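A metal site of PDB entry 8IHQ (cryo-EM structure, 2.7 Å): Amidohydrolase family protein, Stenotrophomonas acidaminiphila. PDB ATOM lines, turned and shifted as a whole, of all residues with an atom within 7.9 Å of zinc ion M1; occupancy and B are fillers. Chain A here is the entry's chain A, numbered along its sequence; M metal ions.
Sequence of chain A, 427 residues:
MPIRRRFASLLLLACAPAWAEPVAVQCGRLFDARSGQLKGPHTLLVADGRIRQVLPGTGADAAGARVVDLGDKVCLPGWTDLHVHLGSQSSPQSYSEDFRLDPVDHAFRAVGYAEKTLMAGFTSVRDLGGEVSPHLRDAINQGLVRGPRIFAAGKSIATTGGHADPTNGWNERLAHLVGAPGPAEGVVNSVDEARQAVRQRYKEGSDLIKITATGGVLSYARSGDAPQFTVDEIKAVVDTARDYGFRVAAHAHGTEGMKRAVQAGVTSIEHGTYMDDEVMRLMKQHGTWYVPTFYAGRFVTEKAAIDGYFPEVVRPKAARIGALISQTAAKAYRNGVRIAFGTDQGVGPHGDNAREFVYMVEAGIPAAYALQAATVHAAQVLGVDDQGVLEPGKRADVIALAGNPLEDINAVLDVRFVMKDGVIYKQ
O of His 83 sits at hydrogen-bond distance from OG1 of Thr 343 (3.3 Å).
The side-chain carboxylate (OD1) of Asp 344 lies close to a ring nitrogen (NE2) of His 85, 3.1 Å away.
A ring nitrogen (ND1) of His 83 sits at hydrogen-bond distance from the side-chain carboxylate (OE1) of Glu 270 (3.1 Å).
O of His 83 lies within hydrogen-bond range of N of Asp 344 (2.6 Å).
NZ of KCX 210 lies within hydrogen-bond range of O of Leu 128, 3.2 Å away.
O of His 83 sits at hydrogen-bond distance from N of Gln 345.
The backbone NH (N) of His 85 sits at hydrogen-bond distance from the backbone carbonyl oxygen (O) of Gln 345 (2.7 Å).
Asp 344 touches zinc ion M1 (OD1 to ZN, 3.1 Å).
Four residues have an atom within 4 Å of zinc ion M1: His 83, His 85, KCX 210 and Asp 344.
The nearest printed residue that does not touch zinc ion M1 is Leu 128 (4.7 Å).
Zinc ion M1 is bound by OQ1 of KCX 210, 2.1 Å away.
Zinc ion M1 is bound by a ring nitrogen (NE2) of His 83 (2.3 Å).
Zinc ion M1 is bound by a ring nitrogen (NE2) of His 85 (2.3 Å).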
ATOM      1  N   HIS A  83      -4.866  29.529 -15.067  1.00  0.00           N
ATOM      2  CA  HIS A  83      -3.534  29.466 -14.489  1.00  0.00           C
ATOM      3  C   HIS A  83      -2.642  28.671 -15.453  1.00  0.00           C
ATOM      4  O   HIS A  83      -2.689  27.448 -15.466  1.00  0.00           O
ATOM      5  CB  HIS A  83      -3.560  28.824 -13.111  1.00  0.00           C
ATOM      6  CG  HIS A  83      -2.361  29.132 -12.270  1.00  0.00           C
ATOM      7  ND1 HIS A  83      -2.367  29.004 -10.901  1.00  0.00           N
ATOM      8  CD2 HIS A  83      -1.125  29.560 -12.601  1.00  0.00           C
ATOM      9  CE1 HIS A  83      -1.180  29.341 -10.424  1.00  0.00           C
ATOM     10  NE2 HIS A  83      -0.406  29.672 -11.442  1.00  0.00           N
ATOM     11  N   VAL A  84      -1.855  29.399 -16.258  1.00  0.00           N
ATOM     12  CA  VAL A  84      -0.890  28.794 -17.161  1.00  0.00           C
ATOM     13  C   VAL A  84       0.392  29.617 -17.132  1.00  0.00           C
ATOM     14  O   VAL A  84       0.413  30.760 -16.693  1.00  0.00           O
ATOM     15  CB  VAL A  84      -1.407  28.689 -18.631  1.00  0.00           C
ATOM     16  CG1 VAL A  84      -2.763  27.998 -18.683  1.00  0.00           C
ATOM     17  CG2 VAL A  84      -1.478  30.060 -19.261  1.00  0.00           C
ATOM     18  N   HIS A  85       1.472  28.997 -17.627  1.00  0.00           N
ATOM     19  CA  HIS A  85       2.763  29.672 -17.822  1.00  0.00           C
ATOM     20  C   HIS A  85       3.251  29.261 -19.208  1.00  0.00           C
ATOM     21  O   HIS A  85       3.965  28.276 -19.355  1.00  0.00           O
ATOM     22  CB  HIS A  85       3.762  29.304 -16.727  1.00  0.00           C
ATOM     23  CG  HIS A  85       3.285  29.608 -15.352  1.00  0.00           C
ATOM     24  ND1 HIS A  85       3.433  30.858 -14.770  1.00  0.00           N
ATOM     25  CD2 HIS A  85       2.655  28.845 -14.431  1.00  0.00           C
ATOM     26  CE1 HIS A  85       2.917  30.840 -13.561  1.00  0.00           C
ATOM     27  NE2 HIS A  85       2.440  29.627 -13.319  1.00  0.00           N
ATOM     28  N   ASP A 127      -2.413  34.075 -18.068  1.00  0.00           N
ATOM     29  CA  ASP A 127      -1.032  33.802 -17.732  1.00  0.00           C
ATOM     30  C   ASP A 127      -0.663  34.545 -16.449  1.00  0.00           C
ATOM     31  O   ASP A 127      -0.880  35.761 -16.341  1.00  0.00           O
ATOM     32  CB  ASP A 127      -0.110  34.234 -18.877  1.00  0.00           C
ATOM     33  CG  ASP A 127       1.291  33.697 -18.727  1.00  0.00           C
ATOM     34  OD1 ASP A 127       2.047  34.228 -17.880  1.00  0.00           O
ATOM     35  OD2 ASP A 127       1.648  32.745 -19.446  1.00  0.00           O
ATOM     36  N   LEU A 128      -0.113  33.818 -15.482  1.00  0.00           N
ATOM     37  CA  LEU A 128       0.097  34.324 -14.133  1.00  0.00           C
ATOM     38  C   LEU A 128       1.587  34.400 -13.806  1.00  0.00           C
ATOM     39  O   LEU A 128       2.026  34.028 -12.718  1.00  0.00           O
ATOM     40  CB  LEU A 128      -0.621  33.455 -13.106  1.00  0.00           C
ATOM     41  CG  LEU A 128      -2.129  33.708 -12.930  1.00  0.00           C
ATOM     42  CD1 LEU A 128      -2.640  32.977 -11.703  1.00  0.00           C
ATOM     43  CD2 LEU A 128      -2.436  35.190 -12.845  1.00  0.00           C
ATOM     44  N   GLY A 129       2.389  34.889 -14.745  1.00  0.00           N
ATOM     45  CA  GLY A 129       3.812  35.055 -14.516  1.00  0.00           C
ATOM     46  C   GLY A 129       4.662  34.812 -15.743  1.00  0.00           C
ATOM     47  O   GLY A 129       4.498  33.805 -16.428  1.00  0.00           O
ATOM     48  N   HIS A 163       8.833  33.793  -3.006  1.00  0.00           N
ATOM     49  CA  HIS A 163       8.658  32.742  -3.991  1.00  0.00           C
ATOM     50  C   HIS A 163       8.968  33.217  -5.403  1.00  0.00           C
ATOM     51  O   HIS A 163       9.475  32.445  -6.219  1.00  0.00           O
ATOM     52  CB  HIS A 163       7.236  32.179  -3.915  1.00  0.00           C
ATOM     53  CG  HIS A 163       6.977  31.041  -4.856  1.00  0.00           C
ATOM     54  ND1 HIS A 163       7.725  29.884  -4.847  1.00  0.00           N
ATOM     55  CD2 HIS A 163       6.054  30.879  -5.825  1.00  0.00           C
ATOM     56  CE1 HIS A 163       7.286  29.065  -5.774  1.00  0.00           C
ATOM     57  NE2 HIS A 163       6.269  29.649  -6.387  1.00  0.00           N
ATOM     58  N   KCX A 210      -0.298  39.849 -10.003  1.00  0.00           N
ATOM     59  CA  KCX A 210      -0.013  38.567  -9.357  1.00  0.00           C
ATOM     60  CB  KCX A 210       0.559  37.573 -10.377  1.00  0.00           C
ATOM     61  CG  KCX A 210       0.051  36.144 -10.251  1.00  0.00           C
ATOM     62  CD  KCX A 210       0.325  35.547  -8.887  1.00  0.00           C
ATOM     63  CE  KCX A 210       0.083  34.055  -8.885  1.00  0.00           C
ATOM     64  NZ  KCX A 210       1.117  33.348  -9.684  1.00  0.00           N
ATOM     65  C   KCX A 210       0.956  38.738  -8.195  1.00  0.00           C
ATOM     66  O   KCX A 210       2.063  39.267  -8.373  1.00  0.00           O
ATOM     67  CX  KCX A 210       1.302  32.036  -9.527  1.00  0.00           C
ATOM     68  OQ1 KCX A 210       2.173  31.457 -10.203  1.00  0.00           O
ATOM     69  OQ2 KCX A 210       0.614  31.404  -8.720  1.00  0.00           O
ATOM     70  N   THR A 212       2.739  36.679  -4.645  1.00  0.00           N
ATOM     71  CA  THR A 212       2.985  35.438  -3.913  1.00  0.00           C
ATOM     72  C   THR A 212       2.783  35.723  -2.427  1.00  0.00           C
ATOM     73  O   THR A 212       3.631  36.364  -1.792  1.00  0.00           O
ATOM     74  CB  THR A 212       4.391  34.913  -4.184  1.00  0.00           C
ATOM     75  OG1 THR A 212       5.350  35.936  -3.906  1.00  0.00           O
ATOM     76  CG2 THR A 212       4.531  34.472  -5.632  1.00  0.00           C
ATOM     77  N   LEU A 218       8.443  25.143  -5.844  1.00  0.00           N
ATOM     78  CA  LEU A 218       9.453  25.046  -6.897  1.00  0.00           C
ATOM     79  C   LEU A 218      10.538  26.109  -6.793  1.00  0.00           C
ATOM     80  O   LEU A 218      11.475  26.089  -7.588  1.00  0.00           O
ATOM     81  CB  LEU A 218       8.775  25.113  -8.267  1.00  0.00           C
ATOM     82  CG  LEU A 218       7.976  23.882  -8.685  1.00  0.00           C
ATOM     83  CD1 LEU A 218       7.282  24.117 -10.016  1.00  0.00           C
ATOM     84  CD2 LEU A 218       8.857  22.653  -8.754  1.00  0.00           C
ATOM     85  N   HIS A 251      -0.939  33.609  -4.955  1.00  0.00           N
ATOM     86  CA  HIS A 251      -0.469  32.223  -4.757  1.00  0.00           C
ATOM     87  C   HIS A 251      -0.310  31.999  -3.249  1.00  0.00           C
ATOM     88  O   HIS A 251       0.377  32.809  -2.622  1.00  0.00           O
ATOM     89  CB  HIS A 251       0.859  32.041  -5.507  1.00  0.00           C
ATOM     90  CG  HIS A 251       1.811  31.082  -4.875  1.00  0.00           C
ATOM     91  ND1 HIS A 251       2.152  29.884  -5.482  1.00  0.00           N
ATOM     92  CD2 HIS A 251       2.522  31.146  -3.729  1.00  0.00           C
ATOM     93  CE1 HIS A 251       3.012  29.251  -4.715  1.00  0.00           C
ATOM     94  NE2 HIS A 251       3.249  29.993  -3.636  1.00  0.00           N
ATOM     95  N   GLU A 270      -4.728  31.004  -5.512  1.00  0.00           N
ATOM     96  CA  GLU A 270      -4.182  30.077  -6.499  1.00  0.00           C
ATOM     97  C   GLU A 270      -3.967  28.672  -5.940  1.00  0.00           C
ATOM     98  O   GLU A 270      -4.031  27.699  -6.701  1.00  0.00           O
ATOM     99  CB  GLU A 270      -2.860  30.611  -7.065  1.00  0.00           C
ATOM    100  CG  GLU A 270      -3.014  31.775  -8.031  1.00  0.00           C
ATOM    101  CD  GLU A 270      -4.309  31.733  -8.825  1.00  0.00           C
ATOM    102  OE1 GLU A 270      -4.575  30.714  -9.502  1.00  0.00           O
ATOM    103  OE2 GLU A 270      -5.064  32.724  -8.775  1.00  0.00           O
ATOM    104  N   HIS A 271      -3.687  28.530  -4.651  1.00  0.00           N
ATOM    105  CA  HIS A 271      -3.617  27.222  -4.021  1.00  0.00           C
ATOM    106  C   HIS A 271      -4.193  27.321  -2.626  1.00  0.00           C
ATOM    107  O   HIS A 271      -4.281  28.400  -2.037  1.00  0.00           O
ATOM    108  CB  HIS A 271      -2.178  26.681  -3.981  1.00  0.00           C
ATOM    109  CG  HIS A 271      -1.398  26.899  -5.235  1.00  0.00           C
ATOM    110  ND1 HIS A 271      -1.580  26.149  -6.372  1.00  0.00           N
ATOM    111  CD2 HIS A 271      -0.422  27.795  -5.537  1.00  0.00           C
ATOM    112  CE1 HIS A 271      -0.758  26.559  -7.318  1.00  0.00           C
ATOM    113  NE2 HIS A 271      -0.047  27.563  -6.830  1.00  0.00           N
ATOM    114  N   THR A 293      -5.982  23.568  -9.027  1.00  0.00           N
ATOM    115  CA  THR A 293      -4.810  23.110  -9.794  1.00  0.00           C
ATOM    116  C   THR A 293      -4.356  21.727  -9.317  1.00  0.00           C
ATOM    117  O   THR A 293      -3.286  21.546  -8.744  1.00  0.00           O
ATOM    118  CB  THR A 293      -3.653  24.113  -9.716  1.00  0.00           C
ATOM    119  OG1 THR A 293      -3.013  24.018  -8.433  1.00  0.00           O
ATOM    120  CG2 THR A 293      -4.137  25.539  -9.940  1.00  0.00           C
ATOM    121  N   ALA A 296      -0.912  20.318 -11.256  1.00  0.00           N
ATOM    122  CA  ALA A 296       0.419  20.684 -10.772  1.00  0.00           C
ATOM    123  C   ALA A 296       0.810  19.860  -9.549  1.00  0.00           C
ATOM    124  O   ALA A 296       1.956  19.421  -9.441  1.00  0.00           O
ATOM    125  CB  ALA A 296       0.468  22.176 -10.454  1.00  0.00           C
ATOM    126  N   THR A 343      -5.035  25.149 -14.232  1.00  0.00           N
ATOM    127  CA  THR A 343      -4.177  23.976 -14.341  1.00  0.00           C
ATOM    128  C   THR A 343      -2.757  24.184 -13.842  1.00  0.00           C
ATOM    129  O   THR A 343      -2.120  23.203 -13.453  1.00  0.00           O
ATOM    130  CB  THR A 343      -4.105  23.505 -15.800  1.00  0.00           C
ATOM    131  OG1 THR A 343      -3.816  24.618 -16.652  1.00  0.00           O
ATOM    132  CG2 THR A 343      -5.403  22.866 -16.234  1.00  0.00           C
ATOM    133  N   ASP A 344      -2.241  25.415 -13.869  1.00  0.00           N
ATOM    134  CA  ASP A 344      -0.838  25.701 -13.564  1.00  0.00           C
ATOM    135  C   ASP A 344       0.093  24.992 -14.548  1.00  0.00           C
ATOM    136  O   ASP A 344       1.123  24.431 -14.175  1.00  0.00           O
ATOM    137  CB  ASP A 344      -0.485  25.321 -12.121  1.00  0.00           C
ATOM    138  CG  ASP A 344       0.752  26.043 -11.622  1.00  0.00           C
ATOM    139  OD1 ASP A 344       1.322  26.851 -12.373  1.00  0.00           O
ATOM    140  OD2 ASP A 344       1.159  25.796 -10.458  1.00  0.00           O
ATOM    141  N   GLN A 345      -0.280  25.013 -15.827  1.00  0.00           N
ATOM    142  CA  GLN A 345       0.575  24.430 -16.849  1.00  0.00           C
ATOM    143  C   GLN A 345       1.841  25.267 -17.014  1.00  0.00           C
ATOM    144  O   GLN A 345       1.887  26.453 -16.697  1.00  0.00           O
ATOM    145  CB  GLN A 345      -0.164  24.321 -18.190  1.00  0.00           C
ATOM    146  CG  GLN A 345      -1.369  23.408 -18.142  1.00  0.00           C
ATOM    147  CD  GLN A 345      -1.027  21.947 -17.954  1.00  0.00           C
ATOM    148  OE1 GLN A 345      -0.882  21.195 -18.921  1.00  0.00           O
ATOM    149  NE2 GLN A 345      -0.897  21.519 -16.703  1.00  0.00           N
ATOM    150  N   VAL A 347       4.335  23.685 -15.355  1.00  0.00           N
ATOM    151  CA  VAL A 347       4.808  22.521 -14.621  1.00  0.00           C
ATOM    152  C   VAL A 347       4.514  21.245 -15.418  1.00  0.00           C
ATOM    153  O   VAL A 347       5.408  20.451 -15.721  1.00  0.00           O
ATOM    154  CB  VAL A 347       4.181  22.466 -13.222  1.00  0.00           C
ATOM    155  CG1 VAL A 347       4.821  21.382 -12.385  1.00  0.00           C
ATOM    156  CG2 VAL A 347       4.306  23.812 -12.531  1.00  0.00           C
HETATM  157 ZN    ZN M   1       1.863  29.585 -11.093  1.00  0.00          ZN
HETATM  158 ZN    ZN M   2       1.456  29.232  -7.362  1.00  0.00          ZN
